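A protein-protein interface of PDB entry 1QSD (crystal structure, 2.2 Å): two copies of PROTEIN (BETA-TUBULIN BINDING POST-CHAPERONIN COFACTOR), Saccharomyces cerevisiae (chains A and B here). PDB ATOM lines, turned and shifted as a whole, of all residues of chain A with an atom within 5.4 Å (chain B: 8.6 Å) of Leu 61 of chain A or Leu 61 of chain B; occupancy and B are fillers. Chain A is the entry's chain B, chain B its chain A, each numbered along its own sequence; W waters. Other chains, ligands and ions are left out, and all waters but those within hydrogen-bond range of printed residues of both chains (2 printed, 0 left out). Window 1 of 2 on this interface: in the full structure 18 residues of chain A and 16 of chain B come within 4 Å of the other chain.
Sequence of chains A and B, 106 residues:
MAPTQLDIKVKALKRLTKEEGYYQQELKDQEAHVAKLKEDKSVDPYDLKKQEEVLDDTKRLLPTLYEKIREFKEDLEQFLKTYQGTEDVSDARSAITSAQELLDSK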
ATOM      1  N   GLU A  19      17.973  -1.442  10.671  1.00  0.00           N
ATOM      2  CA  GLU A  19      17.416  -0.644  11.755  1.00  0.00           C
ATOM      3  C   GLU A  19      18.388   0.470  12.176  1.00  0.00           C
ATOM      4  O   GLU A  19      17.976   1.582  12.507  1.00  0.00           O
ATOM      5  CB  GLU A  19      17.084  -1.541  12.936  1.00  0.00           C
ATOM      6  CG  GLU A  19      17.052  -0.830  14.270  1.00  0.00           C
ATOM      7  CD  GLU A  19      16.603  -1.723  15.406  1.00  0.00           C
ATOM      8  OE1 GLU A  19      16.485  -1.218  16.549  1.00  0.00           O
ATOM      9  OE2 GLU A  19      16.362  -2.929  15.165  1.00  0.00           O
ATOM     10  N   TYR A  23      17.514   4.374  12.429  1.00  0.00           N
ATOM     11  CA  TYR A  23      17.752   5.217  13.594  1.00  0.00           C
ATOM     12  C   TYR A  23      18.754   6.337  13.299  1.00  0.00           C
ATOM     13  O   TYR A  23      18.665   7.425  13.884  1.00  0.00           O
ATOM     14  CB  TYR A  23      18.233   4.388  14.792  1.00  0.00           C
ATOM     15  CG  TYR A  23      17.165   3.502  15.406  1.00  0.00           C
ATOM     16  CD1 TYR A  23      16.108   3.008  14.636  1.00  0.00           C
ATOM     17  CD2 TYR A  23      17.205   3.153  16.759  1.00  0.00           C
ATOM     18  CE1 TYR A  23      15.118   2.185  15.195  1.00  0.00           C
ATOM     19  CE2 TYR A  23      16.209   2.325  17.332  1.00  0.00           C
ATOM     20  CZ  TYR A  23      15.174   1.852  16.542  1.00  0.00           C
ATOM     21  OH  TYR A  23      14.172   1.047  17.045  1.00  0.00           O
ATOM     22  N   ASP A  57      18.563  11.320  24.206  1.00  0.00           N
ATOM     23  CA  ASP A  57      17.859  10.050  24.349  1.00  0.00           C
ATOM     24  C   ASP A  57      18.058   9.194  23.110  1.00  0.00           C
ATOM     25  O   ASP A  57      18.483   8.046  23.201  1.00  0.00           O
ATOM     26  CB  ASP A  57      16.378  10.291  24.599  1.00  0.00           C
ATOM     27  CG  ASP A  57      16.097  10.682  26.028  1.00  0.00           C
ATOM     28  OD1 ASP A  57      15.086  10.219  26.578  1.00  0.00           O
ATOM     29  OD2 ASP A  57      16.889  11.439  26.626  1.00  0.00           O
ATOM     30  N   THR A  58      17.779   9.774  21.953  1.00  0.00           N
ATOM     31  CA  THR A  58      17.952   9.082  20.698  1.00  0.00           C
ATOM     32  C   THR A  58      19.382   8.511  20.670  1.00  0.00           C
ATOM     33  O   THR A  58      19.551   7.304  20.567  1.00  0.00           O
ATOM     34  CB  THR A  58      17.727  10.051  19.504  1.00  0.00           C
ATOM     35  OG1 THR A  58      16.444  10.682  19.621  1.00  0.00           O
ATOM     36  CG2 THR A  58      17.791   9.303  18.185  1.00  0.00           C
ATOM     37  N   LYS A  59      20.391   9.360  20.871  1.00  0.00           N
ATOM     38  CA  LYS A  59      21.800   8.937  20.849  1.00  0.00           C
ATOM     39  C   LYS A  59      22.179   7.766  21.757  1.00  0.00           C
ATOM     40  O   LYS A  59      23.024   6.948  21.389  1.00  0.00           O
ATOM     41  CB  LYS A  59      22.731  10.108  21.168  1.00  0.00           C
ATOM     42  CG  LYS A  59      22.928  11.111  20.065  1.00  0.00           C
ATOM     43  CD  LYS A  59      23.851  12.217  20.545  1.00  0.00           C
ATOM     44  CE  LYS A  59      24.152  13.226  19.442  1.00  0.00           C
ATOM     45  NZ  LYS A  59      25.100  14.313  19.876  1.00  0.00           N
ATOM     46  N   ARG A  60      21.577   7.689  22.941  1.00  0.00           N
ATOM     47  CA  ARG A  60      21.881   6.615  23.891  1.00  0.00           C
ATOM     48  C   ARG A  60      21.462   5.228  23.363  1.00  0.00           C
ATOM     49  O   ARG A  60      21.933   4.189  23.840  1.00  0.00           O
ATOM     50  CB  ARG A  60      21.217   6.906  25.240  1.00  0.00           C
ATOM     51  CG  ARG A  60      19.920   6.147  25.486  1.00  0.00           C
ATOM     52  CD  ARG A  60      18.925   6.943  26.312  1.00  0.00           C
ATOM     53  NE  ARG A  60      19.540   7.556  27.491  1.00  0.00           N
ATOM     54  CZ  ARG A  60      18.991   8.548  28.193  1.00  0.00           C
ATOM     55  NH1 ARG A  60      17.807   9.039  27.847  1.00  0.00           N
ATOM     56  NH2 ARG A  60      19.640   9.067  29.227  1.00  0.00           N
ATOM     57  N   LEU A  61      20.596   5.232  22.356  1.00  0.00           N
ATOM     58  CA  LEU A  61      20.088   4.023  21.719  1.00  0.00           C
ATOM     59  C   LEU A  61      21.161   3.314  20.866  1.00  0.00           C
ATOM     60  O   LEU A  61      21.207   2.079  20.791  1.00  0.00           O
ATOM     61  CB  LEU A  61      18.936   4.433  20.809  1.00  0.00           C
ATOM     62  CG  LEU A  61      17.596   3.717  20.740  1.00  0.00           C
ATOM     63  CD1 LEU A  61      16.708   4.539  19.817  1.00  0.00           C
ATOM     64  CD2 LEU A  61      17.746   2.284  20.220  1.00  0.00           C
ATOM     65  N   LEU A  62      22.018   4.096  20.216  1.00  0.00           N
ATOM     66  CA  LEU A  62      23.037   3.535  19.337  1.00  0.00           C
ATOM     67  C   LEU A  62      24.078   2.605  19.954  1.00  0.00           C
ATOM     68  O   LEU A  62      24.349   1.535  19.403  1.00  0.00           O
ATOM     69  CB  LEU A  62      23.721   4.630  18.511  1.00  0.00           C
ATOM     70  CG  LEU A  62      22.840   5.308  17.457  1.00  0.00           C
ATOM     71  CD1 LEU A  62      23.733   6.135  16.529  1.00  0.00           C
ATOM     72  CD2 LEU A  62      22.061   4.265  16.650  1.00  0.00           C
ATOM     73  N   PRO A  63      24.645   2.961  21.115  1.00  0.00           N
ATOM     74  CA  PRO A  63      25.649   2.086  21.723  1.00  0.00           C
ATOM     75  C   PRO A  63      25.218   0.619  21.835  1.00  0.00           C
ATOM     76  O   PRO A  63      25.939  -0.283  21.420  1.00  0.00           O
ATOM     77  CB  PRO A  63      25.850   2.709  23.108  1.00  0.00           C
ATOM     78  CG  PRO A  63      25.603   4.115  22.872  1.00  0.00           C
ATOM     79  CD  PRO A  63      24.396   4.126  21.979  1.00  0.00           C
ATOM     80  N   THR A  64      24.039   0.386  22.400  1.00  0.00           N
ATOM     81  CA  THR A  64      23.536  -0.964  22.573  1.00  0.00           C
ATOM     82  C   THR A  64      23.209  -1.594  21.238  1.00  0.00           C
ATOM     83  O   THR A  64      23.288  -2.805  21.075  1.00  0.00           O
ATOM     84  CB  THR A  64      22.285  -0.988  23.460  1.00  0.00           C
ATOM     85  OG1 THR A  64      21.363   0.006  23.006  1.00  0.00           O
ATOM     86  CG2 THR A  64      22.653  -0.703  24.908  1.00  0.00           C
ATOM     87  N   LEU A  65      22.814  -0.779  20.282  1.00  0.00           N
ATOM     88  CA  LEU A  65      22.523  -1.318  18.981  1.00  0.00           C
ATOM     89  C   LEU A  65      23.824  -1.886  18.366  1.00  0.00           C
ATOM     90  O   LEU A  65      23.821  -3.012  17.865  1.00  0.00           O
ATOM     91  CB  LEU A  65      21.861  -0.244  18.110  1.00  0.00           C
ATOM     92  CG  LEU A  65      21.332  -0.600  16.728  1.00  0.00           C
ATOM     93  CD1 LEU A  65      20.629  -1.941  16.724  1.00  0.00           C
ATOM     94  CD2 LEU A  65      20.417   0.515  16.245  1.00  0.00           C
ATOM     95  N   GLU B  19       7.105  10.968  15.818  1.00  0.00           N
ATOM     96  CA  GLU B  19       8.196  10.029  16.125  1.00  0.00           C
ATOM     97  C   GLU B  19       7.629   8.740  16.764  1.00  0.00           C
ATOM     98  O   GLU B  19       8.012   7.626  16.395  1.00  0.00           O
ATOM     99  CB  GLU B  19       9.211  10.689  17.064  1.00  0.00           C
ATOM    100  CG  GLU B  19      10.209   9.728  17.688  1.00  0.00           C
ATOM    101  CD  GLU B  19      11.334  10.420  18.467  1.00  0.00           C
ATOM    102  OE1 GLU B  19      12.156   9.698  19.083  1.00  0.00           O
ATOM    103  OE2 GLU B  19      11.414  11.671  18.453  1.00  0.00           O
ATOM    104  N   GLU B  20       6.698   8.898  17.703  1.00  0.00           N
ATOM    105  CA  GLU B  20       6.047   7.775  18.378  1.00  0.00           C
ATOM    106  C   GLU B  20       5.412   6.845  17.350  1.00  0.00           C
ATOM    107  O   GLU B  20       5.446   5.625  17.502  1.00  0.00           O
ATOM    108  CB  GLU B  20       4.961   8.302  19.323  1.00  0.00           C
ATOM    109  CG  GLU B  20       4.306   7.263  20.211  1.00  0.00           C
ATOM    110  CD  GLU B  20       3.031   6.662  19.621  1.00  0.00           C
ATOM    111  OE1 GLU B  20       2.562   7.094  18.547  1.00  0.00           O
ATOM    112  OE2 GLU B  20       2.478   5.746  20.259  1.00  0.00           O
ATOM    113  N   TYR B  23       8.216   4.884  15.614  1.00  0.00           N
ATOM    114  CA  TYR B  23       8.705   3.833  16.495  1.00  0.00           C
ATOM    115  C   TYR B  23       7.661   2.725  16.686  1.00  0.00           C
ATOM    116  O   TYR B  23       8.009   1.553  16.851  1.00  0.00           O
ATOM    117  CB  TYR B  23       9.119   4.429  17.844  1.00  0.00           C
ATOM    118  CG  TYR B  23      10.441   5.189  17.845  1.00  0.00           C
ATOM    119  CD1 TYR B  23      10.896   5.885  16.714  1.00  0.00           C
ATOM    120  CD2 TYR B  23      11.239   5.212  18.988  1.00  0.00           C
ATOM    121  CE1 TYR B  23      12.131   6.587  16.729  1.00  0.00           C
ATOM    122  CE2 TYR B  23      12.459   5.901  19.013  1.00  0.00           C
ATOM    123  CZ  TYR B  23      12.905   6.585  17.894  1.00  0.00           C
ATOM    124  OH  TYR B  23      14.123   7.237  18.008  1.00  0.00           O
ATOM    125  N   GLN B  24       6.384   3.087  16.631  1.00  0.00           N
ATOM    126  CA  GLN B  24       5.314   2.114  16.789  1.00  0.00           C
ATOM    127  C   GLN B  24       5.227   1.183  15.577  1.00  0.00           C
ATOM    128  O   GLN B  24       4.714   0.073  15.686  1.00  0.00           O
ATOM    129  CB  GLN B  24       3.974   2.815  17.024  1.00  0.00           C
ATOM    130  CG  GLN B  24       3.037   2.100  18.022  1.00  0.00           C
ATOM    131  CD  GLN B  24       3.449   2.254  19.490  1.00  0.00           C
ATOM    132  OE1 GLN B  24       3.196   1.373  20.311  1.00  0.00           O
ATOM    133  NE2 GLN B  24       4.061   3.382  19.824  1.00  0.00           N
ATOM    134  N   GLU B  26       8.005   0.202  13.781  1.00  0.00           N
ATOM    135  CA  GLU B  26       9.165  -0.661  13.983  1.00  0.00           C
ATOM    136  C   GLU B  26       8.791  -1.783  14.940  1.00  0.00           C
ATOM    137  O   GLU B  26       9.002  -2.954  14.640  1.00  0.00           O
ATOM    138  CB  GLU B  26      10.322   0.151  14.572  1.00  0.00           C
ATOM    139  CG  GLU B  26      11.607   0.137  13.742  1.00  0.00           C
ATOM    140  CD  GLU B  26      12.577  -0.981  14.125  1.00  0.00           C
ATOM    141  OE1 GLU B  26      12.706  -1.961  13.352  1.00  0.00           O
ATOM    142  OE2 GLU B  26      13.225  -0.868  15.195  1.00  0.00           O
ATOM    143  N   LEU B  27       8.207  -1.411  16.076  1.00  0.00           N
ATOM    144  CA  LEU B  27       7.787  -2.354  17.102  1.00  0.00           C
ATOM    145  C   LEU B  27       6.827  -3.413  16.566  1.00  0.00           C
ATOM    146  O   LEU B  27       6.997  -4.606  16.827  1.00  0.00           O
ATOM    147  CB  LEU B  27       7.125  -1.604  18.258  1.00  0.00           C
ATOM    148  CG  LEU B  27       6.851  -2.422  19.522  1.00  0.00           C
ATOM    149  CD1 LEU B  27       8.173  -2.889  20.139  1.00  0.00           C
ATOM    150  CD2 LEU B  27       6.081  -1.584  20.521  1.00  0.00           C
ATOM    151  N   GLN B  30       8.592  -5.929  14.323  1.00  0.00           N
ATOM    152  CA  GLN B  30       9.466  -6.829  15.070  1.00  0.00           C
ATOM    153  C   GLN B  30       8.689  -7.952  15.769  1.00  0.00           C
ATOM    154  O   GLN B  30       9.165  -9.089  15.845  1.00  0.00           O
ATOM    155  CB  GLN B  30      10.315  -6.055  16.083  1.00  0.00           C
ATOM    156  CG  GLN B  30      11.479  -5.287  15.464  1.00  0.00           C
ATOM    157  CD  GLN B  30      12.328  -4.566  16.498  1.00  0.00           C
ATOM    158  OE1 GLN B  30      12.820  -5.173  17.449  1.00  0.00           O
ATOM    159  NE2 GLN B  30      12.497  -3.271  16.321  1.00  0.00           N
ATOM    160  N   VAL B  54      16.123  -8.200  21.155  1.00  0.00           N
ATOM    161  CA  VAL B  54      16.071  -6.975  20.357  1.00  0.00           C
ATOM    162  C   VAL B  54      14.706  -6.326  20.518  1.00  0.00           C
ATOM    163  O   VAL B  54      14.608  -5.108  20.727  1.00  0.00           O
ATOM    164  CB  VAL B  54      16.374  -7.222  18.853  1.00  0.00           C
ATOM    165  CG1 VAL B  54      16.014  -5.992  18.019  1.00  0.00           C
ATOM    166  CG2 VAL B  54      17.854  -7.534  18.662  1.00  0.00           C
ATOM    167  N   LEU B  55      13.649  -7.134  20.469  1.00  0.00           N
ATOM    168  CA  LEU B  55      12.312  -6.588  20.627  1.00  0.00           C
ATOM    169  C   LEU B  55      12.210  -5.835  21.957  1.00  0.00           C
ATOM    170  O   LEU B  55      11.766  -4.691  21.983  1.00  0.00           O
ATOM    171  CB  LEU B  55      11.242  -7.694  20.546  1.00  0.00           C
ATOM    172  CG  LEU B  55       9.785  -7.209  20.667  1.00  0.00           C
ATOM    173  CD1 LEU B  55       9.442  -6.311  19.504  1.00  0.00           C
ATOM    174  CD2 LEU B  55       8.818  -8.368  20.727  1.00  0.00           C
ATOM    175  N   ASP B  56      12.691  -6.461  23.035  1.00  0.00           N
ATOM    176  CA  ASP B  56      12.649  -5.877  24.382  1.00  0.00           C
ATOM    177  C   ASP B  56      13.317  -4.516  24.426  1.00  0.00           C
ATOM    178  O   ASP B  56      12.878  -3.636  25.158  1.00  0.00           O
ATOM    179  CB  ASP B  56      13.319  -6.796  25.422  1.00  0.00           C
ATOM    180  CG  ASP B  56      12.568  -8.111  25.655  1.00  0.00           C
ATOM    181  OD1 ASP B  56      13.104  -8.968  26.380  1.00  0.00           O
ATOM    182  OD2 ASP B  56      11.453  -8.302  25.125  1.00  0.00           O
ATOM    183  N   ASP B  57      14.404  -4.359  23.681  1.00  0.00           N
ATOM    184  CA  ASP B  57      15.114  -3.096  23.641  1.00  0.00           C
ATOM    185  C   ASP B  57      14.233  -2.038  23.000  1.00  0.00           C
ATOM    186  O   ASP B  57      14.012  -0.970  23.575  1.00  0.00           O
ATOM    187  CB  ASP B  57      16.434  -3.245  22.887  1.00  0.00           C
ATOM    188  CG  ASP B  57      17.518  -3.848  23.745  1.00  0.00           C
ATOM    189  OD1 ASP B  57      18.693  -3.438  23.600  1.00  0.00           O
ATOM    190  OD2 ASP B  57      17.195  -4.720  24.583  1.00  0.00           O
ATOM    191  N   THR B  58      13.710  -2.353  21.820  1.00  0.00           N
ATOM    192  CA  THR B  58      12.823  -1.456  21.100  1.00  0.00           C
ATOM    193  C   THR B  58      11.723  -0.976  22.052  1.00  0.00           C
ATOM    194  O   THR B  58      11.503   0.216  22.198  1.00  0.00           O
ATOM    195  CB  THR B  58      12.194  -2.184  19.906  1.00  0.00           C
ATOM    196  OG1 THR B  58      13.238  -2.703  19.071  1.00  0.00           O
ATOM    197  CG2 THR B  58      11.326  -1.242  19.092  1.00  0.00           C
ATOM    198  N   LYS B  59      11.075  -1.903  22.739  1.00  0.00           N
ATOM    199  CA  LYS B  59      10.025  -1.550  23.684  1.00  0.00           C
ATOM    200  C   LYS B  59      10.449  -0.563  24.782  1.00  0.00           C
ATOM    201  O   LYS B  59       9.691   0.349  25.113  1.00  0.00           O
ATOM    202  CB  LYS B  59       9.448  -2.809  24.341  1.00  0.00           C
ATOM    203  CG  LYS B  59       8.568  -3.657  23.450  1.00  0.00           C
ATOM    204  CD  LYS B  59       8.082  -4.889  24.195  1.00  0.00           C
ATOM    205  CE  LYS B  59       7.061  -5.665  23.374  1.00  0.00           C
ATOM    206  NZ  LYS B  59       6.560  -6.879  24.095  1.00  0.00           N
ATOM    207  N   ARG B  60      11.650  -0.721  25.331  1.00  0.00           N
ATOM    208  CA  ARG B  60      12.125   0.148  26.414  1.00  0.00           C
ATOM    209  C   ARG B  60      12.127   1.643  26.028  1.00  0.00           C
ATOM    210  O   ARG B  60      11.994   2.535  26.875  1.00  0.00           O
ATOM    211  CB  ARG B  60      13.512  -0.337  26.895  1.00  0.00           C
ATOM    212  CG  ARG B  60      14.729   0.461  26.380  1.00  0.00           C
ATOM    213  CD  ARG B  60      16.037  -0.351  26.330  1.00  0.00           C
ATOM    214  NE  ARG B  60      16.252  -1.204  27.499  1.00  0.00           N
ATOM    215  CZ  ARG B  60      16.986  -2.312  27.482  1.00  0.00           C
ATOM    216  NH1 ARG B  60      17.579  -2.695  26.360  1.00  0.00           N
ATOM    217  NH2 ARG B  60      17.088  -3.071  28.566  1.00  0.00           N
ATOM    218  N   LEU B  61      12.192   1.885  24.726  1.00  0.00           N
ATOM    219  CA  LEU B  61      12.211   3.223  24.136  1.00  0.00           C
ATOM    220  C   LEU B  61      10.884   3.980  24.230  1.00  0.00           C
ATOM    221  O   LEU B  61      10.859   5.214  24.235  1.00  0.00           O
ATOM    222  CB  LEU B  61      12.554   3.088  22.660  1.00  0.00           C
ATOM    223  CG  LEU B  61      13.649   3.903  22.007  1.00  0.00           C
ATOM    224  CD1 LEU B  61      13.739   3.410  20.586  1.00  0.00           C
ATOM    225  CD2 LEU B  61      13.341   5.387  22.053  1.00  0.00           C
ATOM    226  N   LEU B  62       9.779   3.245  24.227  1.00  0.00           N
ATOM    227  CA  LEU B  62       8.461   3.859  24.277  1.00  0.00           C
ATOM    228  C   LEU B  62       8.081   4.594  25.542  1.00  0.00           C
ATOM    229  O   LEU B  62       7.590   5.719  25.464  1.00  0.00           O
ATOM    230  CB  LEU B  62       7.379   2.854  23.914  1.00  0.00           C
ATOM    231  CG  LEU B  62       7.402   2.482  22.435  1.00  0.00           C
ATOM    232  CD1 LEU B  62       6.178   1.668  22.103  1.00  0.00           C
ATOM    233  CD2 LEU B  62       7.437   3.745  21.581  1.00  0.00           C
ATOM    234  N   PRO B  63       8.317   3.993  26.723  1.00  0.00           N
ATOM    235  CA  PRO B  63       7.957   4.681  27.961  1.00  0.00           C
ATOM    236  C   PRO B  63       8.536   6.091  28.056  1.00  0.00           C
ATOM    237  O   PRO B  63       7.790   7.047  28.228  1.00  0.00           O
ATOM    238  CB  PRO B  63       8.530   3.765  29.042  1.00  0.00           C
ATOM    239  CG  PRO B  63       8.453   2.429  28.424  1.00  0.00           C
ATOM    240  CD  PRO B  63       8.938   2.690  27.024  1.00  0.00           C
ATOM    241  N   THR B  64       9.847   6.226  27.875  1.00  0.00           N
ATOM    242  CA  THR B  64      10.491   7.530  27.986  1.00  0.00           C
ATOM    243  C   THR B  64       9.961   8.507  26.967  1.00  0.00           C
ATOM    244  O   THR B  64       9.915   9.720  27.215  1.00  0.00           O
ATOM    245  CB  THR B  64      12.025   7.423  27.873  1.00  0.00           C
ATOM    246  OG1 THR B  64      12.360   6.525  26.808  1.00  0.00           O
ATOM    247  CG2 THR B  64      12.631   6.920  29.207  1.00  0.00           C
ATOM    248  N   LEU B  65       9.520   7.956  25.841  1.00  0.00           N
ATOM    249  CA  LEU B  65       8.957   8.736  24.746  1.00  0.00           C
ATOM    250  C   LEU B  65       7.584   9.287  25.131  1.00  0.00           C
ATOM    251  O   LEU B  65       7.249  10.427  24.770  1.00  0.00           O
ATOM    252  CB  LEU B  65       8.859   7.880  23.487  1.00  0.00           C
ATOM    253  CG  LEU B  65       8.390   8.566  22.215  1.00  0.00           C
ATOM    254  CD1 LEU B  65       9.208   9.831  21.952  1.00  0.00           C
ATOM    255  CD2 LEU B  65       8.519   7.608  21.088  1.00  0.00           C
ATOM    256  N   TYR B  66       6.799   8.497  25.876  1.00  0.00           N
ATOM    257  CA  TYR B  66       5.483   8.952  26.330  1.00  0.00           C
ATOM    258  C   TYR B  66       5.630  10.001  27.405  1.00  0.00           C
ATOM    259  O   TYR B  66       4.831  10.929  27.452  1.00  0.00           O
ATOM    260  CB  TYR B  66       4.634   7.813  26.852  1.00  0.00           C
ATOM    261  CG  TYR B  66       4.205   6.868  25.769  1.00  0.00           C
ATOM    262  CD1 TYR B  66       3.460   7.316  24.669  1.00  0.00           C
ATOM    263  CD2 TYR B  66       4.545   5.522  25.831  1.00  0.00           C
ATOM    264  CE1 TYR B  66       3.063   6.436  23.657  1.00  0.00           C
ATOM    265  CE2 TYR B  66       4.153   4.635  24.826  1.00  0.00           C
ATOM    266  CZ  TYR B  66       3.416   5.092  23.747  1.00  0.00           C
ATOM    267  OH  TYR B  66       3.023   4.162  22.805  1.00  0.00           O
ATOM    268  N   GLU B  67       6.656   9.857  28.249  1.00  0.00           N
ATOM    269  CA  GLU B  67       6.939  10.820  29.303  1.00  0.00           C
ATOM    270  C   GLU B  67       7.179  12.202  28.664  1.00  0.00           C
ATOM    271  O   GLU B  67       6.594  13.188  29.086  1.00  0.00           O
ATOM    272  CB  GLU B  67       8.176  10.381  30.110  1.00  0.00           C
ATOM    273  CG  GLU B  67       7.924   9.198  31.063  1.00  0.00           C
ATOM    274  CD  GLU B  67       9.212   8.536  31.592  1.00  0.00           C
ATOM    275  OE1 GLU B  67       9.337   7.280  31.517  1.00  0.00           O
ATOM    276  OE2 GLU B  67      10.101   9.272  32.086  1.00  0.00           O
ATOM    277  N   LYS B  68       7.982  12.244  27.602  1.00  0.00           N
ATOM    278  CA  LYS B  68       8.291  13.495  26.906  1.00  0.00           C
ATOM    279  C   LYS B  68       7.128  14.081  26.156  1.00  0.00           C
ATOM    280  O   LYS B  68       7.023  15.290  26.030  1.00  0.00           O
ATOM    281  CB  LYS B  68       9.516  13.348  26.009  1.00  0.00           C
ATOM    282  CG  LYS B  68      10.781  13.259  26.825  1.00  0.00           C
ATOM    283  CD  LYS B  68      11.997  13.249  25.982  1.00  0.00           C
ATOM    284  CE  LYS B  68      13.225  13.049  26.844  1.00  0.00           C
ATOM    285  NZ  LYS B  68      14.442  12.904  25.985  1.00  0.00           N
HETATM  286  O   HOH W   1      14.211  10.082  20.939  1.00  0.00           O
HETATM  287  O   HOH W   2      15.401  12.371  29.251  1.00  0.00           O
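Of chain A, only Leu 61 comes within 4 Å of Leu 61 of chain B.
Printed residues of chain B within 4 Å of Asp 57 of chain A: Lys 68 (2.8 Å).
Printed residues of chain B within 4 Å of Tyr 23 of chain A: Glu 26 (2.8 Å).
Of the printed residues of chain A, Glu 26 of chain B touches Glu 19 (3.5 Å) and Tyr 23 (2.8 Å).
Of the printed residues of chain B, Glu 19 of chain A touches Glu 26 (3.5 Å).
Val 54 of chain B touches none of the printed residues of chain A.
Leu 55 of chain B touches none of the printed residues of chain A.
The nearest residue of chain B that does not touch Leu 61 of chain A is Tyr 23 of chain B (4.2 Å).
The nearest residue of chain A that does not touch Leu 61 of chain B is Tyr 23 of chain A (4.2 Å).
The nearest printed residue of chain B that does not touch Glu 19 of chain A is Gln 30 of chain B (4.05 Å).
Glu 19 of chain A touches Glu 26 of chain B.
Leu 61 of chain B touches Leu 61 of chain A.
Hydrophobic or aromatic side chains of chain A that line the printed part of chain B: Tyr 23 and Leu 61.
Hydrophobic or aromatic side chains of chain B within 4 Å of the printed part of chain A: Leu 61.
Among the printed residues, 4 pairs touch across the chains.
OH of Tyr 23 of chain A is in hydrogen-bond range of OE1 of Glu 19 of chain A, 3.3 Å away.
The side-chain hydroxyl of Thr 64 of chain A is in hydrogen-bond range of the backbone carbonyl oxygen of Leu 61 of chain A (3.0 Å).
The side-chain carboxylate (OD2) of Asp 57 of chain A lies within salt-bridge range of the guanidinium group (NH1) of Arg 60 of chain A, 2.8 Å away.
OG1 of Thr 64 of chain B is in hydrogen-bond range of O of Leu 61 of chain B (3.3 Å).
OE2 of Glu 26 of chain B sits at hydrogen-bond distance from NE2 of Gln 30 of chain B, at 2.8 Å.
Water W1 bridges the side-chain hydroxyl (OG1) of Thr 58 of chain A (2.7 Å) and the side-chain carboxylate (OE1) of Glu 19 of chain B (2.8 Å).
Water W2 bridges the side-chain carboxylate (OD2) of Asp 57 of chain A (3.2 Å) and the side-chain amino group (NZ) of Lys 68 of chain B (3.4 Å).
NZ of Lys 68 of chain B lies within salt-bridge range of OD1 of Asp 57 of chain A, 2.8 Å away.
The side-chain carboxylate (OE2) of Glu 26 of chain B is in hydrogen-bond range of the side-chain hydroxyl (OH) of Tyr 23 of chain A (2.8 Å).
Leu 61 of chain A touches its own counterpart, Leu 61 of chain B.
Positions printed for both chains: 19, 23, 57, 58, 59, 60, 61, 62, 63, 64 and 65.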
